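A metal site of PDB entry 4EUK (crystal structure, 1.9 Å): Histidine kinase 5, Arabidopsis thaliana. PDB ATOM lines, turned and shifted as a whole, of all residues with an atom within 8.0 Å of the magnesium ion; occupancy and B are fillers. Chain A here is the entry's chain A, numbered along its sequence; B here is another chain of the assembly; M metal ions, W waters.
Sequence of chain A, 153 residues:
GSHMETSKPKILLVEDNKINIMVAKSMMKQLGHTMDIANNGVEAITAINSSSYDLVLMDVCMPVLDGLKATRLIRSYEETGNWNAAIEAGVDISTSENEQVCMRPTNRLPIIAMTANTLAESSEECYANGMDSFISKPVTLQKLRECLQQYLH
Water W1 bridges OE2 of Glu 15 (2.4 Å) and NZ of Lys 137 (3.2 Å).
Water W3 bridges OD1 of Asp 59 (2.9 Å) and NZ of Lys 137 (3.3 Å).
Water W2 lies within hydrogen-bond range of the side-chain carboxylate of Asp 16 (2.7 Å) and a ring nitrogen (NE2) of His 84 of chain B (3.3 Å).
OD1 of Asp 59 lies within salt-bridge range of NZ of Lys 137, at 2.7 Å.
The backbone carbonyl oxygen (O) of Val 14 is in hydrogen-bond range of the backbone NH (N) of Asp 59, at 2.8 Å.
The side-chain carboxylate (OE2) of Glu 121 is in hydrogen-bond range of the side-chain sulfur (SG) of Cys 61 (3.2 Å).
OE1 of Glu 15 lies within salt-bridge range of NZ of Lys 137 (3.2 Å).
N of Asn 17 sits at hydrogen-bond distance from OE2 of Glu 15 (2.8 Å).
The side-chain amide oxygen of Asn 20 sits close to the side-chain carboxylate of Glu 15 (3.4 Å).
The backbone carbonyl oxygen (O) of Glu 15 is in hydrogen-bond range of the side-chain amide nitrogen (ND2) of Asn 39, 3.1 Å away.
Merely in contact with the magnesium ion: Glu 15 (3.7 Å).
Four residues have an atom within 4 Å of the magnesium ion: Glu 15, Asp 16, Asp 59 and Cys 61.
Along chain A the residues within 4 Å of the magnesium ion span positions 15 to 61.
The magnesium ion is bound by the side-chain carboxylate of Asp 59 (1.9 Å), the side-chain carboxylate of Asp 16 (2.0 Å), the backbone carbonyl oxygen of Cys 61 (2.0 Å), water W3 (2.1 Å), water W1 (2.1 Å) and water W2 (2.1 Å).
The magnesium ion has six donor atoms within binding distance.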
ATOM      1  N   VAL A  14     -17.434  12.182  19.343  1.00  0.00           N
ATOM      2  CA  VAL A  14     -17.933  11.723  18.043  1.00  0.00           C
ATOM      3  C   VAL A  14     -17.144  12.465  16.976  1.00  0.00           C
ATOM      4  O   VAL A  14     -17.246  13.695  16.828  1.00  0.00           O
ATOM      5  CB  VAL A  14     -19.444  11.979  17.853  1.00  0.00           C
ATOM      6  CG1 VAL A  14     -19.941  11.198  16.647  1.00  0.00           C
ATOM      7  CG2 VAL A  14     -20.248  11.626  19.144  1.00  0.00           C
ATOM      8  N   GLU A  15     -16.338  11.715  16.232  1.00  0.00           N
ATOM      9  CA  GLU A  15     -15.419  12.300  15.273  1.00  0.00           C
ATOM     10  C   GLU A  15     -14.984  11.201  14.302  1.00  0.00           C
ATOM     11  O   GLU A  15     -14.752  10.053  14.693  1.00  0.00           O
ATOM     12  CB  GLU A  15     -14.248  12.954  16.039  1.00  0.00           C
ATOM     13  CG  GLU A  15     -13.036  13.306  15.282  1.00  0.00           C
ATOM     14  CD  GLU A  15     -13.215  14.452  14.310  1.00  0.00           C
ATOM     15  OE1 GLU A  15     -13.318  15.617  14.761  1.00  0.00           O
ATOM     16  OE2 GLU A  15     -13.196  14.180  13.079  1.00  0.00           O
ATOM     17  N   ASP A  16     -14.910  11.556  13.016  1.00  0.00           N
ATOM     18  CA  ASP A  16     -14.572  10.604  11.988  1.00  0.00           C
ATOM     19  C   ASP A  16     -13.106  10.640  11.631  1.00  0.00           C
ATOM     20  O   ASP A  16     -12.610   9.712  11.001  1.00  0.00           O
ATOM     21  CB  ASP A  16     -15.412  10.844  10.731  1.00  0.00           C
ATOM     22  CG  ASP A  16     -15.235  12.233  10.133  1.00  0.00           C
ATOM     23  OD1 ASP A  16     -15.425  13.245  10.840  1.00  0.00           O
ATOM     24  OD2 ASP A  16     -14.938  12.308   8.937  1.00  0.00           O
ATOM     25  N   ASN A  17     -12.390  11.704  11.983  1.00  0.00           N
ATOM     26  CA  ASN A  17     -10.995  11.833  11.574  1.00  0.00           C
ATOM     27  C   ASN A  17     -10.075  11.274  12.657  1.00  0.00           C
ATOM     28  O   ASN A  17     -10.049  11.778  13.773  1.00  0.00           O
ATOM     29  CB  ASN A  17     -10.688  13.295  11.217  1.00  0.00           C
ATOM     30  CG  ASN A  17      -9.245  13.538  10.788  1.00  0.00           C
ATOM     31  OD1 ASN A  17      -8.311  13.103  11.455  1.00  0.00           O
ATOM     32  ND2 ASN A  17      -9.071  14.303   9.693  1.00  0.00           N
ATOM     33  N   ASN A  20      -7.656  13.734  14.329  1.00  0.00           N
ATOM     34  CA  ASN A  20      -8.387  14.567  15.270  1.00  0.00           C
ATOM     35  C   ASN A  20      -8.667  13.801  16.576  1.00  0.00           C
ATOM     36  O   ASN A  20      -8.588  14.359  17.654  1.00  0.00           O
ATOM     37  CB  ASN A  20      -9.718  15.038  14.680  1.00  0.00           C
ATOM     38  CG  ASN A  20      -9.572  16.038  13.524  1.00  0.00           C
ATOM     39  OD1 ASN A  20     -10.586  16.457  12.916  1.00  0.00           O
ATOM     40  ND2 ASN A  20      -8.352  16.424  13.211  1.00  0.00           N
ATOM     41  N   ASN A  39     -17.517   7.076  15.697  1.00  0.00           N
ATOM     42  CA  ASN A  39     -16.945   7.637  14.446  1.00  0.00           C
ATOM     43  C   ASN A  39     -17.973   8.234  13.459  1.00  0.00           C
ATOM     44  O   ASN A  39     -17.593   8.748  12.408  1.00  0.00           O
ATOM     45  CB  ASN A  39     -16.119   6.584  13.744  1.00  0.00           C
ATOM     46  CG  ASN A  39     -14.925   6.098  14.570  1.00  0.00           C
ATOM     47  OD1 ASN A  39     -14.722   4.912  14.731  1.00  0.00           O
ATOM     48  ND2 ASN A  39     -14.135   7.028  15.088  1.00  0.00           N
ATOM     49  N   MET A  58     -19.391  16.672  19.586  1.00  0.00           N
ATOM     50  CA  MET A  58     -19.980  16.154  18.358  1.00  0.00           C
ATOM     51  C   MET A  58     -19.423  16.842  17.136  1.00  0.00           C
ATOM     52  O   MET A  58     -19.716  18.009  16.875  1.00  0.00           O
ATOM     53  CB  MET A  58     -21.515  16.352  18.387  1.00  0.00           C
ATOM     54  CG  MET A  58     -22.280  15.856  17.133  1.00  0.00           C
ATOM     55  SD  MET A  58     -22.550  14.076  17.149  1.00  0.00           S
ATOM     56  CE  MET A  58     -23.939  13.949  18.291  1.00  0.00           C
ATOM     57  N   ASP A  59     -18.656  16.114  16.337  1.00  0.00           N
ATOM     58  CA  ASP A  59     -18.170  16.639  15.077  1.00  0.00           C
ATOM     59  C   ASP A  59     -19.388  16.931  14.201  1.00  0.00           C
ATOM     60  O   ASP A  59     -20.390  16.207  14.248  1.00  0.00           O
ATOM     61  CB  ASP A  59     -17.289  15.596  14.421  1.00  0.00           C
ATOM     62  CG  ASP A  59     -16.564  16.099  13.166  1.00  0.00           C
ATOM     63  OD1 ASP A  59     -16.318  17.315  13.008  1.00  0.00           O
ATOM     64  OD2 ASP A  59     -16.201  15.227  12.368  1.00  0.00           O
ATOM     65  N   VAL A  60     -19.307  17.992  13.412  1.00  0.00           N
ATOM     66  CA  VAL A  60     -20.407  18.352  12.524  1.00  0.00           C
ATOM     67  C   VAL A  60     -20.431  17.511  11.249  1.00  0.00           C
ATOM     68  O   VAL A  60     -21.433  16.867  10.951  1.00  0.00           O
ATOM     69  CB  VAL A  60     -20.404  19.853  12.197  1.00  0.00           C
ATOM     70  CG1 VAL A  60     -21.413  20.188  11.079  1.00  0.00           C
ATOM     71  CG2 VAL A  60     -20.717  20.601  13.450  1.00  0.00           C
ATOM     72  N   CYS A  61     -19.319  17.465  10.525  1.00  0.00           N
ATOM     73  CA  CYS A  61     -19.271  16.764   9.241  1.00  0.00           C
ATOM     74  C   CYS A  61     -18.682  15.371   9.381  1.00  0.00           C
ATOM     75  O   CYS A  61     -17.519  15.206   9.724  1.00  0.00           O
ATOM     76  CB  CYS A  61     -18.488  17.561   8.206  1.00  0.00           C
ATOM     77  SG  CYS A  61     -19.262  19.121   7.692  1.00  0.00           S
ATOM     78  N   MET A  62     -19.513  14.357   9.120  1.00  0.00           N
ATOM     79  CA  MET A  62     -19.150  12.951   9.220  1.00  0.00           C
ATOM     80  C   MET A  62     -19.942  12.177   8.168  1.00  0.00           C
ATOM     81  O   MET A  62     -21.080  12.579   7.854  1.00  0.00           O
ATOM     82  CB  MET A  62     -19.508  12.368  10.597  1.00  0.00           C
ATOM     83  CG  MET A  62     -18.878  13.094  11.792  1.00  0.00           C
ATOM     84  SD  MET A  62     -19.302  12.326  13.372  1.00  0.00           S
ATOM     85  CE  MET A  62     -21.004  12.867  13.633  1.00  0.00           C
ATOM     86  N   PRO A  63     -19.389  11.058   7.680  1.00  0.00           N
ATOM     87  CA  PRO A  63     -20.145  10.158   6.816  1.00  0.00           C
ATOM     88  C   PRO A  63     -21.217   9.346   7.549  1.00  0.00           C
ATOM     89  O   PRO A  63     -21.212   9.259   8.791  1.00  0.00           O
ATOM     90  CB  PRO A  63     -19.077   9.214   6.243  1.00  0.00           C
ATOM     91  CG  PRO A  63     -17.957   9.279   7.191  1.00  0.00           C
ATOM     92  CD  PRO A  63     -18.011  10.589   7.906  1.00  0.00           C
ATOM     93  N   GLY A  67     -23.305  15.219  12.310  1.00  0.00           N
ATOM     94  CA  GLY A  67     -23.564  15.577  13.691  1.00  0.00           C
ATOM     95  C   GLY A  67     -24.771  16.466  13.868  1.00  0.00           C
ATOM     96  O   GLY A  67     -25.343  16.503  14.957  1.00  0.00           O
ATOM     97  N   MET A 114     -18.206  20.532  17.163  1.00  0.00           N
ATOM     98  CA  MET A 114     -16.821  20.868  16.740  1.00  0.00           C
ATOM     99  C   MET A 114     -16.917  21.238  15.242  1.00  0.00           C
ATOM    100  O   MET A 114     -17.329  20.428  14.408  1.00  0.00           O
ATOM    101  CB  MET A 114     -15.877  19.708  17.015  1.00  0.00           C
ATOM    102  CG  MET A 114     -15.776  19.294  18.470  1.00  0.00           C
ATOM    103  SD  MET A 114     -14.707  17.867  18.847  1.00  0.00           S
ATOM    104  CE  MET A 114     -15.699  16.565  18.075  1.00  0.00           C
ATOM    105  N   ALA A 116     -15.725  23.325  11.517  1.00  0.00           N
ATOM    106  CA  ALA A 116     -14.590  23.324  10.587  1.00  0.00           C
ATOM    107  C   ALA A 116     -14.404  24.585   9.730  1.00  0.00           C
ATOM    108  O   ALA A 116     -13.771  24.521   8.660  1.00  0.00           O
ATOM    109  CB  ALA A 116     -14.701  22.118   9.675  1.00  0.00           C
ATOM    110  N   GLU A 121     -21.051  25.246   8.414  1.00  0.00           N
ATOM    111  CA  GLU A 121     -20.870  24.976   9.840  1.00  0.00           C
ATOM    112  C   GLU A 121     -20.861  26.226  10.705  1.00  0.00           C
ATOM    113  O   GLU A 121     -20.094  26.300  11.640  1.00  0.00           O
ATOM    114  CB  GLU A 121     -19.610  24.143  10.084  1.00  0.00           C
ATOM    115  CG  GLU A 121     -19.533  22.904   9.196  1.00  0.00           C
ATOM    116  CD  GLU A 121     -18.237  22.135   9.295  1.00  0.00           C
ATOM    117  OE1 GLU A 121     -17.794  21.814  10.421  1.00  0.00           O
ATOM    118  OE2 GLU A 121     -17.666  21.809   8.227  1.00  0.00           O
ATOM    119  N   LYS A 137     -12.555  24.246  15.315  1.00  0.00           N
ATOM    120  CA  LYS A 137     -11.351  23.440  15.131  1.00  0.00           C
ATOM    121  C   LYS A 137     -10.233  24.315  14.604  1.00  0.00           C
ATOM    122  O   LYS A 137     -10.487  25.282  13.915  1.00  0.00           O
ATOM    123  CB  LYS A 137     -11.598  22.303  14.153  1.00  0.00           C
ATOM    124  CG  LYS A 137     -12.493  21.230  14.705  1.00  0.00           C
ATOM    125  CD  LYS A 137     -12.880  20.295  13.541  1.00  0.00           C
ATOM    126  CE  LYS A 137     -13.525  19.032  13.955  1.00  0.00           C
ATOM    127  NZ  LYS A 137     -13.770  18.099  12.798  1.00  0.00           N
ATOM    128  N   HIS B  84     -11.270  17.516   2.024  1.00  0.00           N
ATOM    129  CA  HIS B  84     -11.783  17.868   3.335  1.00  0.00           C
ATOM    130  C   HIS B  84     -10.983  17.179   4.434  1.00  0.00           C
ATOM    131  O   HIS B  84     -10.628  17.812   5.421  1.00  0.00           O
ATOM    132  CB  HIS B  84     -13.272  17.493   3.431  1.00  0.00           C
ATOM    133  CG  HIS B  84     -13.909  17.787   4.749  1.00  0.00           C
ATOM    134  ND1 HIS B  84     -14.804  18.814   4.927  1.00  0.00           N
ATOM    135  CD2 HIS B  84     -13.780  17.192   5.958  1.00  0.00           C
ATOM    136  CE1 HIS B  84     -15.197  18.844   6.181  1.00  0.00           C
ATOM    137  NE2 HIS B  84     -14.589  17.866   6.840  1.00  0.00           N
ATOM    138  N   GLN B  85     -10.726  15.893   4.284  1.00  0.00           N
ATOM    139  CA  GLN B  85      -9.992  15.118   5.314  1.00  0.00           C
ATOM    140  C   GLN B  85      -8.553  15.637   5.450  1.00  0.00           C
ATOM    141  O   GLN B  85      -8.050  15.783   6.567  1.00  0.00           O
ATOM    142  CB  GLN B  85     -10.068  13.600   5.010  1.00  0.00           C
ATOM    143  CG  GLN B  85      -9.042  12.680   5.747  1.00  0.00           C
ATOM    144  CD  GLN B  85      -9.581  11.911   6.963  1.00  0.00           C
ATOM    145  OE1 GLN B  85     -10.721  12.069   7.403  1.00  0.00           O
ATOM    146  NE2 GLN B  85      -8.717  11.032   7.513  1.00  0.00           N
ATOM    147  N   GLY B  88      -8.535  18.932   7.341  1.00  0.00           N
ATOM    148  CA  GLY B  88      -8.748  18.729   8.776  1.00  0.00           C
ATOM    149  C   GLY B  88      -7.502  18.200   9.490  1.00  0.00           C
ATOM    150  O   GLY B  88      -7.158  18.680  10.594  1.00  0.00           O
HETATM  151 MG    MG M   1     -15.637  15.235  10.504  1.00  0.00          MG
HETATM  152  O   HOH W   1     -13.639  15.458  11.078  1.00  0.00           O
HETATM  153  O   HOH W   2     -15.081  14.980   8.463  1.00  0.00           O
HETATM  154  O   HOH W   3     -15.662  17.277  10.170  1.00  0.00           O
